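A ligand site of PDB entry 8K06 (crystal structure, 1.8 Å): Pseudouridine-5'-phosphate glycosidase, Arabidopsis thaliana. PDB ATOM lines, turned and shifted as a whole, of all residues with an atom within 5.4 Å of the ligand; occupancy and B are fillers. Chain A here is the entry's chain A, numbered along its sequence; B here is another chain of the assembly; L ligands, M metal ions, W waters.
Water W3 bridges an oxygen (O5) of the ligand (2.5 Å) and the side-chain amino group (NZ) of Lys 112 (2.7 Å). Water W2 lies within hydrogen-bond range of O8 of the ligand (2.6 Å), OG1 of Thr 289 (2.8 Å) and O of Gly 285 (3.4 Å). Water W5 lies within hydrogen-bond range of OE2 of Glu 198 of chain B (2.5 Å), O8 of the ligand (2.7 Å) and N of Asn 286 (3.4 Å). Water W6 bridges a ring nitrogen (NE2) of His 156 (2.7 Å) and an oxygen (O9) of the ligand (2.7 Å). Water W1 lies within hydrogen-bond range of the side-chain carboxylate of Asp 168 (2.6 Å), the side-chain hydroxyl of Thr 131 (2.7 Å), the side-chain hydroxyl of Ser 133 (2.8 Å), an oxygen (O7) of the ligand (2.8 Å) and the side-chain hydroxyl of Ser 167 (3.4 Å). Water W4 lies within hydrogen-bond range of the backbone NH of Ser 167 (3.0 Å), an oxygen (O7) of the ligand (3.2 Å) and the side-chain carboxylate of Glu 198 of chain B (3.3 Å).
O of Asn 286 is in hydrogen-bond range of NZ of Lys 112. The side-chain hydroxyl of Thr 149 lies within hydrogen-bond range of the backbone carbonyl oxygen of Gly 151 (3.5 Å). O of Gly 154 sits at hydrogen-bond distance from N of Ser 166 (2.9 Å). OG1 of Thr 52 lies within hydrogen-bond range of OE1 of Glu 50, at 2.5 Å. OE2 of Glu 50 is in hydrogen-bond range of OG1 of Thr 149 (2.5 Å). N of Asp 168 lies close to OG of Ser 166 (3.1 Å). OD2 of Asp 168 sits at hydrogen-bond distance from N of Gly 153. OG1 of Thr 131 is in hydrogen-bond range of OG of Ser 133, at 3.2 Å.
N of Val 132 sits at hydrogen-bond distance from O4 of the ligand (2.8 Å). The side-chain amino group (NZ) of Lys 112 lies within salt-bridge range of an oxygen (O8) of the ligand (3.1 Å). An oxygen (O1) of the ligand is in hydrogen-bond range of the side-chain amide nitrogen (ND2) of Asn 308, 3.1 Å away. OG of Ser 166 sits at hydrogen-bond distance from O9 of the ligand. The side-chain carboxylate of Asp 168 is in hydrogen-bond range of an oxygen (O4) of the ligand (2.6 Å). An oxygen (O3) of the ligand lies within hydrogen-bond range of the side-chain carboxylate (OE1) of Glu 50, at 2.6 Å.
O2 of the ligand sits close to O of Gly 151, 3.4 Å away. Thr 52 touches the ligand (OG1 to O3, 3.5 Å). Thr 131 touches the ligand. Gly 153 touches the ligand (CA to C9, 3.9 Å). Asn 286 touches the ligand. CD1 of Leu 293 touches O1 of the ligand, 3.2 Å away. Hydrophobic or aromatic side chains that line the ligand: Val 132 and Leu 293. Of the 26 residues printed, 12 come within 4 Å of the ligand.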
ATOM      1  N   GLU A  50     -31.919  10.762 -27.566  1.00  0.00           N
ATOM      2  CA  GLU A  50     -30.790   9.838 -27.547  1.00  0.00           C
ATOM      3  C   GLU A  50     -30.855   8.950 -26.304  1.00  0.00           C
ATOM      4  O   GLU A  50     -31.658   9.183 -25.410  1.00  0.00           O
ATOM      5  CB  GLU A  50     -29.471  10.615 -27.655  1.00  0.00           C
ATOM      6  CG  GLU A  50     -29.217  11.566 -26.538  1.00  0.00           C
ATOM      7  CD  GLU A  50     -27.790  12.040 -26.502  1.00  0.00           C
ATOM      8  OE1 GLU A  50     -26.855  11.190 -26.496  1.00  0.00           O
ATOM      9  OE2 GLU A  50     -27.601  13.265 -26.477  1.00  0.00           O
ATOM     10  N   THR A  52     -27.783   7.763 -24.535  1.00  0.00           N
ATOM     11  CA  THR A  52     -26.551   7.730 -23.731  1.00  0.00           C
ATOM     12  C   THR A  52     -26.703   8.171 -22.277  1.00  0.00           C
ATOM     13  O   THR A  52     -25.964   7.681 -21.430  1.00  0.00           O
ATOM     14  CB  THR A  52     -25.433   8.618 -24.353  1.00  0.00           C
ATOM     15  OG1 THR A  52     -25.942   9.935 -24.582  1.00  0.00           O
ATOM     16  CG2 THR A  52     -24.892   8.041 -25.654  1.00  0.00           C
ATOM     17  N   ILE A  53     -27.636   9.071 -21.960  1.00  0.00           N
ATOM     18  CA  ILE A  53     -27.860   9.409 -20.551  1.00  0.00           C
ATOM     19  C   ILE A  53     -28.429   8.228 -19.793  1.00  0.00           C
ATOM     20  O   ILE A  53     -28.156   8.048 -18.597  1.00  0.00           O
ATOM     21  CB  ILE A  53     -28.772  10.637 -20.370  1.00  0.00           C
ATOM     22  CG1 ILE A  53     -28.033  11.907 -20.759  1.00  0.00           C
ATOM     23  CG2 ILE A  53     -29.195  10.780 -18.913  1.00  0.00           C
ATOM     24  CD1 ILE A  53     -28.867  13.168 -20.679  1.00  0.00           C
ATOM     25  N   LYS A 112     -20.836   3.268 -26.374  1.00  0.00           N
ATOM     26  CA  LYS A 112     -21.021   4.663 -26.784  1.00  0.00           C
ATOM     27  C   LYS A 112     -20.810   4.716 -28.285  1.00  0.00           C
ATOM     28  O   LYS A 112     -19.730   4.396 -28.776  1.00  0.00           O
ATOM     29  CB  LYS A 112     -20.027   5.593 -26.067  1.00  0.00           C
ATOM     30  CG  LYS A 112     -20.055   7.012 -26.601  1.00  0.00           C
ATOM     31  CD  LYS A 112     -19.102   7.926 -25.837  1.00  0.00           C
ATOM     32  CE  LYS A 112     -18.916   9.254 -26.566  1.00  0.00           C
ATOM     33  NZ  LYS A 112     -18.049  10.205 -25.810  1.00  0.00           N
ATOM     34  N   ALA A 114     -20.861   6.766 -31.647  1.00  0.00           N
ATOM     35  CA  ALA A 114     -20.903   7.951 -32.493  1.00  0.00           C
ATOM     36  C   ALA A 114     -21.314   7.560 -33.923  1.00  0.00           C
ATOM     37  O   ALA A 114     -21.435   6.379 -34.238  1.00  0.00           O
ATOM     38  CB  ALA A 114     -19.560   8.664 -32.479  1.00  0.00           C
ATOM     39  N   THR A 130     -26.573   5.689 -28.897  1.00  0.00           N
ATOM     40  CA  THR A 130     -26.165   6.609 -29.942  1.00  0.00           C
ATOM     41  C   THR A 130     -25.961   8.021 -29.376  1.00  0.00           C
ATOM     42  O   THR A 130     -26.808   8.540 -28.641  1.00  0.00           O
ATOM     43  CB  THR A 130     -27.189   6.630 -31.085  1.00  0.00           C
ATOM     44  OG1 THR A 130     -28.509   6.762 -30.546  1.00  0.00           O
ATOM     45  CG2 THR A 130     -27.112   5.330 -31.854  1.00  0.00           C
ATOM     46  N   THR A 131     -24.828   8.628 -29.731  1.00  0.00           N
ATOM     47  CA  THR A 131     -24.508  10.008 -29.347  1.00  0.00           C
ATOM     48  C   THR A 131     -25.297  10.966 -30.216  1.00  0.00           C
ATOM     49  O   THR A 131     -26.071  10.536 -31.071  1.00  0.00           O
ATOM     50  CB  THR A 131     -23.001  10.314 -29.525  1.00  0.00           C
ATOM     51  OG1 THR A 131     -22.678  10.261 -30.921  1.00  0.00           O
ATOM     52  CG2 THR A 131     -22.138   9.321 -28.804  1.00  0.00           C
ATOM     53  N   VAL A 132     -25.063  12.268 -30.040  1.00  0.00           N
ATOM     54  CA  VAL A 132     -25.716  13.246 -30.915  1.00  0.00           C
ATOM     55  C   VAL A 132     -25.422  12.999 -32.407  1.00  0.00           C
ATOM     56  O   VAL A 132     -26.353  13.029 -33.234  1.00  0.00           O
ATOM     57  CB  VAL A 132     -25.319  14.676 -30.528  1.00  0.00           C
ATOM     58  CG1 VAL A 132     -25.703  15.659 -31.637  1.00  0.00           C
ATOM     59  CG2 VAL A 132     -25.995  15.036 -29.217  1.00  0.00           C
ATOM     60  N   SER A 133     -24.168  12.739 -32.753  1.00  0.00           N
ATOM     61  CA  SER A 133     -23.847  12.562 -34.176  1.00  0.00           C
ATOM     62  C   SER A 133     -24.534  11.308 -34.771  1.00  0.00           C
ATOM     63  O   SER A 133     -25.019  11.352 -35.910  1.00  0.00           O
ATOM     64  CB  SER A 133     -22.325  12.456 -34.392  1.00  0.00           C
ATOM     65  OG  SER A 133     -21.795  11.290 -33.777  1.00  0.00           O
ATOM     66  N   THR A 149     -31.703  16.939 -26.975  1.00  0.00           N
ATOM     67  CA  THR A 149     -30.550  16.360 -26.298  1.00  0.00           C
ATOM     68  C   THR A 149     -30.345  17.136 -24.999  1.00  0.00           C
ATOM     69  O   THR A 149     -31.185  17.964 -24.647  1.00  0.00           O
ATOM     70  CB  THR A 149     -29.300  16.424 -27.192  1.00  0.00           C
ATOM     71  OG1 THR A 149     -28.247  15.637 -26.617  1.00  0.00           O
ATOM     72  CG2 THR A 149     -28.862  17.866 -27.357  1.00  0.00           C
ATOM     73  N   GLY A 151     -26.780  18.392 -23.845  1.00  0.00           N
ATOM     74  CA  GLY A 151     -25.760  19.276 -24.377  1.00  0.00           C
ATOM     75  C   GLY A 151     -25.188  18.629 -25.618  1.00  0.00           C
ATOM     76  O   GLY A 151     -25.339  17.427 -25.848  1.00  0.00           O
ATOM     77  N   ILE A 152     -24.552  19.427 -26.453  1.00  0.00           N
ATOM     78  CA  ILE A 152     -23.902  18.892 -27.630  1.00  0.00           C
ATOM     79  C   ILE A 152     -22.376  18.857 -27.384  1.00  0.00           C
ATOM     80  O   ILE A 152     -21.861  19.616 -26.562  1.00  0.00           O
ATOM     81  CB  ILE A 152     -24.296  19.707 -28.868  1.00  0.00           C
ATOM     82  CG1 ILE A 152     -23.884  19.016 -30.169  1.00  0.00           C
ATOM     83  CG2 ILE A 152     -23.749  21.140 -28.795  1.00  0.00           C
ATOM     84  CD1 ILE A 152     -24.499  19.709 -31.378  1.00  0.00           C
ATOM     85  N   GLY A 153     -21.689  17.911 -28.012  1.00  0.00           N
ATOM     86  CA  GLY A 153     -20.233  17.868 -27.969  1.00  0.00           C
ATOM     87  C   GLY A 153     -19.657  19.097 -28.647  1.00  0.00           C
ATOM     88  O   GLY A 153     -20.378  19.812 -29.323  1.00  0.00           O
ATOM     89  N   GLY A 154     -18.374  19.372 -28.468  1.00  0.00           N
ATOM     90  CA  GLY A 154     -17.826  20.574 -29.040  1.00  0.00           C
ATOM     91  C   GLY A 154     -16.337  20.479 -29.259  1.00  0.00           C
ATOM     92  O   GLY A 154     -15.762  19.390 -29.357  1.00  0.00           O
ATOM     93  N   HIS A 156     -12.823  20.668 -27.822  1.00  0.00           N
ATOM     94  CA  HIS A 156     -12.276  20.443 -26.485  1.00  0.00           C
ATOM     95  C   HIS A 156     -11.251  21.519 -26.124  1.00  0.00           C
ATOM     96  O   HIS A 156     -10.748  22.248 -26.967  1.00  0.00           O
ATOM     97  CB  HIS A 156     -11.637  19.044 -26.391  1.00  0.00           C
ATOM     98  CG  HIS A 156     -12.654  17.941 -26.331  1.00  0.00           C
ATOM     99  ND1 HIS A 156     -12.905  17.217 -25.182  1.00  0.00           N
ATOM    100  CD2 HIS A 156     -13.513  17.467 -27.267  1.00  0.00           C
ATOM    101  CE1 HIS A 156     -13.860  16.342 -25.413  1.00  0.00           C
ATOM    102  NE2 HIS A 156     -14.252  16.472 -26.669  1.00  0.00           N
ATOM    103  N   ILE A 165     -12.089  17.432 -31.536  1.00  0.00           N
ATOM    104  CA  ILE A 165     -13.322  18.168 -31.826  1.00  0.00           C
ATOM    105  C   ILE A 165     -14.472  17.174 -32.089  1.00  0.00           C
ATOM    106  O   ILE A 165     -14.322  16.233 -32.871  1.00  0.00           O
ATOM    107  CB  ILE A 165     -13.169  19.090 -33.037  1.00  0.00           C
ATOM    108  CG1 ILE A 165     -12.059  20.127 -32.785  1.00  0.00           C
ATOM    109  CG2 ILE A 165     -14.509  19.765 -33.374  1.00  0.00           C
ATOM    110  CD1 ILE A 165     -11.807  21.025 -33.973  1.00  0.00           C
ATOM    111  N   SER A 166     -15.603  17.365 -31.424  1.00  0.00           N
ATOM    112  CA  SER A 166     -16.684  16.370 -31.496  1.00  0.00           C
ATOM    113  C   SER A 166     -17.233  16.250 -32.904  1.00  0.00           C
ATOM    114  O   SER A 166     -17.454  17.260 -33.576  1.00  0.00           O
ATOM    115  CB  SER A 166     -17.827  16.725 -30.541  1.00  0.00           C
ATOM    116  OG  SER A 166     -18.855  15.726 -30.608  1.00  0.00           O
ATOM    117  N   SER A 167     -17.490  15.020 -33.352  1.00  0.00           N
ATOM    118  CA  SER A 167     -18.171  14.808 -34.632  1.00  0.00           C
ATOM    119  C   SER A 167     -19.615  15.306 -34.594  1.00  0.00           C
ATOM    120  O   SER A 167     -20.232  15.464 -35.640  1.00  0.00           O
ATOM    121  CB  SER A 167     -18.141  13.318 -35.024  1.00  0.00           C
ATOM    122  OG  SER A 167     -18.837  12.519 -34.097  1.00  0.00           O
ATOM    123  N   ASP A 168     -20.162  15.602 -33.405  1.00  0.00           N
ATOM    124  CA  ASP A 168     -21.469  16.244 -33.347  1.00  0.00           C
ATOM    125  C   ASP A 168     -21.487  17.504 -34.192  1.00  0.00           C
ATOM    126  O   ASP A 168     -22.490  17.809 -34.828  1.00  0.00           O
ATOM    127  CB  ASP A 168     -21.870  16.663 -31.913  1.00  0.00           C
ATOM    128  CG  ASP A 168     -22.047  15.494 -30.975  1.00  0.00           C
ATOM    129  OD1 ASP A 168     -21.991  14.295 -31.393  1.00  0.00           O
ATOM    130  OD2 ASP A 168     -22.270  15.776 -29.776  1.00  0.00           O
ATOM    131  N   PHE A 215     -25.010  24.841 -20.511  1.00  0.00           N
ATOM    132  CA  PHE A 215     -25.380  23.504 -20.012  1.00  0.00           C
ATOM    133  C   PHE A 215     -25.845  23.581 -18.534  1.00  0.00           C
ATOM    134  O   PHE A 215     -27.004  23.931 -18.273  1.00  0.00           O
ATOM    135  CB  PHE A 215     -24.179  22.564 -20.218  1.00  0.00           C
ATOM    136  CG  PHE A 215     -24.490  21.089 -20.082  1.00  0.00           C
ATOM    137  CD1 PHE A 215     -25.412  20.464 -20.907  1.00  0.00           C
ATOM    138  CD2 PHE A 215     -23.780  20.317 -19.160  1.00  0.00           C
ATOM    139  CE1 PHE A 215     -25.659  19.102 -20.779  1.00  0.00           C
ATOM    140  CE2 PHE A 215     -24.023  18.968 -19.034  1.00  0.00           C
ATOM    141  CZ  PHE A 215     -24.975  18.350 -19.842  1.00  0.00           C
ATOM    142  N   GLY A 285      -9.767  10.593 -26.334  1.00  0.00           N
ATOM    143  CA  GLY A 285     -10.800  10.137 -27.251  1.00  0.00           C
ATOM    144  C   GLY A 285     -12.207  10.197 -26.688  1.00  0.00           C
ATOM    145  O   GLY A 285     -12.562  11.100 -25.928  1.00  0.00           O
ATOM    146  N   ASN A 286     -13.012   9.212 -27.043  1.00  0.00           N
ATOM    147  CA  ASN A 286     -14.422   9.225 -26.687  1.00  0.00           C
ATOM    148  C   ASN A 286     -14.652   8.962 -25.209  1.00  0.00           C
ATOM    149  O   ASN A 286     -15.788   9.008 -24.755  1.00  0.00           O
ATOM    150  CB  ASN A 286     -15.204   8.221 -27.541  1.00  0.00           C
ATOM    151  CG  ASN A 286     -14.800   6.789 -27.268  1.00  0.00           C
ATOM    152  OD1 ASN A 286     -13.727   6.538 -26.704  1.00  0.00           O
ATOM    153  ND2 ASN A 286     -15.645   5.833 -27.668  1.00  0.00           N
ATOM    154  N   THR A 289     -15.235  13.002 -22.456  1.00  0.00           N
ATOM    155  CA  THR A 289     -16.465  13.635 -21.993  1.00  0.00           C
ATOM    156  C   THR A 289     -17.205  12.855 -20.902  1.00  0.00           C
ATOM    157  O   THR A 289     -17.606  13.422 -19.877  1.00  0.00           O
ATOM    158  CB  THR A 289     -17.420  13.908 -23.165  1.00  0.00           C
ATOM    159  OG1 THR A 289     -16.806  14.890 -24.025  1.00  0.00           O
ATOM    160  CG2 THR A 289     -18.766  14.431 -22.651  1.00  0.00           C
ATOM    161  N   LEU A 293     -17.810  14.393 -17.047  1.00  0.00           N
ATOM    162  CA  LEU A 293     -19.158  14.603 -16.511  1.00  0.00           C
ATOM    163  C   LEU A 293     -19.387  13.756 -15.277  1.00  0.00           C
ATOM    164  O   LEU A 293     -19.965  14.235 -14.293  1.00  0.00           O
ATOM    165  CB  LEU A 293     -20.206  14.288 -17.575  1.00  0.00           C
ATOM    166  CG  LEU A 293     -20.264  15.267 -18.755  1.00  0.00           C
ATOM    167  CD1 LEU A 293     -21.337  14.814 -19.741  1.00  0.00           C
ATOM    168  CD2 LEU A 293     -20.565  16.677 -18.269  1.00  0.00           C
ATOM    169  N   ASN A 308     -28.306  18.392 -14.923  1.00  0.00           N
ATOM    170  CA  ASN A 308     -28.354  17.705 -16.216  1.00  0.00           C
ATOM    171  C   ASN A 308     -29.755  17.147 -16.489  1.00  0.00           C
ATOM    172  O   ASN A 308     -30.301  17.279 -17.589  1.00  0.00           O
ATOM    173  CB  ASN A 308     -27.310  16.576 -16.248  1.00  0.00           C
ATOM    174  CG  ASN A 308     -26.972  16.097 -17.671  1.00  0.00           C
ATOM    175  OD1 ASN A 308     -27.766  16.219 -18.618  1.00  0.00           O
ATOM    176  ND2 ASN A 308     -25.771  15.583 -17.825  1.00  0.00           N
ATOM    177  N   GLU B 198     -11.793  11.073 -36.712  1.00  0.00           N
ATOM    178  CA  GLU B 198     -12.968  10.947 -35.852  1.00  0.00           C
ATOM    179  C   GLU B 198     -13.952  12.094 -36.059  1.00  0.00           C
ATOM    180  O   GLU B 198     -15.169  11.863 -36.147  1.00  0.00           O
ATOM    181  CB  GLU B 198     -12.558  10.877 -34.372  1.00  0.00           C
ATOM    182  CG  GLU B 198     -13.779  10.721 -33.464  1.00  0.00           C
ATOM    183  CD  GLU B 198     -13.422  10.524 -31.994  1.00  0.00           C
ATOM    184  OE1 GLU B 198     -12.205  10.474 -31.665  1.00  0.00           O
ATOM    185  OE2 GLU B 198     -14.361  10.429 -31.175  1.00  0.00           O
HETATM  186  N1  LIG L   1     -23.859  12.267 -21.580  1.00  0.00           N
HETATM  187  C1  LIG L   1     -24.017  13.664 -21.142  1.00  0.00           C
HETATM  188  N2  LIG L   1     -23.743  14.765 -22.103  1.00  0.00           N
HETATM  189  C2  LIG L   1     -23.328  14.478 -23.435  1.00  0.00           C
HETATM  190  C3  LIG L   1     -23.163  13.076 -23.843  1.00  0.00           C
HETATM  191  C4  LIG L   1     -23.442  11.988 -22.901  1.00  0.00           C
HETATM  192  O1  LIG L   1     -24.380  13.874 -19.993  1.00  0.00           O
HETATM  193  O2  LIG L   1     -23.097  15.387 -24.219  1.00  0.00           O
HETATM  194  C5  LIG L   1     -22.753  12.686 -25.165  1.00  0.00           C
HETATM  195  C6  LIG L   1     -23.703  13.266 -26.245  1.00  0.00           C
HETATM  196  O3  LIG L   1     -24.506  12.261 -26.821  1.00  0.00           O
HETATM  197  C7  LIG L   1     -22.744  13.948 -27.235  1.00  0.00           C
HETATM  198  C8  LIG L   1     -21.423  13.257 -26.947  1.00  0.00           C
HETATM  199  O4  LIG L   1     -23.153  13.632 -28.570  1.00  0.00           O
HETATM  200  O5  LIG L   1     -21.445  13.064 -25.526  1.00  0.00           O
HETATM  201  C9  LIG L   1     -20.173  13.997 -27.351  1.00  0.00           C
HETATM  202  O6  LIG L   1     -19.046  13.147 -27.155  1.00  0.00           O
HETATM  203  P1  LIG L   1     -17.999  12.867 -28.328  1.00  0.00           P
HETATM  204  O7  LIG L   1     -18.637  11.938 -29.352  1.00  0.00           O
HETATM  205  O8  LIG L   1     -16.780  12.316 -27.618  1.00  0.00           O
HETATM  206  O9  LIG L   1     -17.647  14.162 -28.991  1.00  0.00           O
HETATM  207 MN    MN M   1     -13.233  13.614 -29.170  1.00  0.00          MN
HETATM  208  O   HOH W   1     -20.674  12.016 -31.332  1.00  0.00           O
HETATM  209  O   HOH W   2     -15.490  12.815 -25.372  1.00  0.00           O
HETATM  210  O   HOH W   3     -19.898  11.494 -24.344  1.00  0.00           O
HETATM  211  O   HOH W   4     -16.674  12.632 -31.823  1.00  0.00           O
HETATM  212  O   HOH W   5     -14.525  11.633 -28.945  1.00  0.00           O
HETATM  213  O   HOH W   6     -15.008  14.870 -28.714  1.00  0.00           O
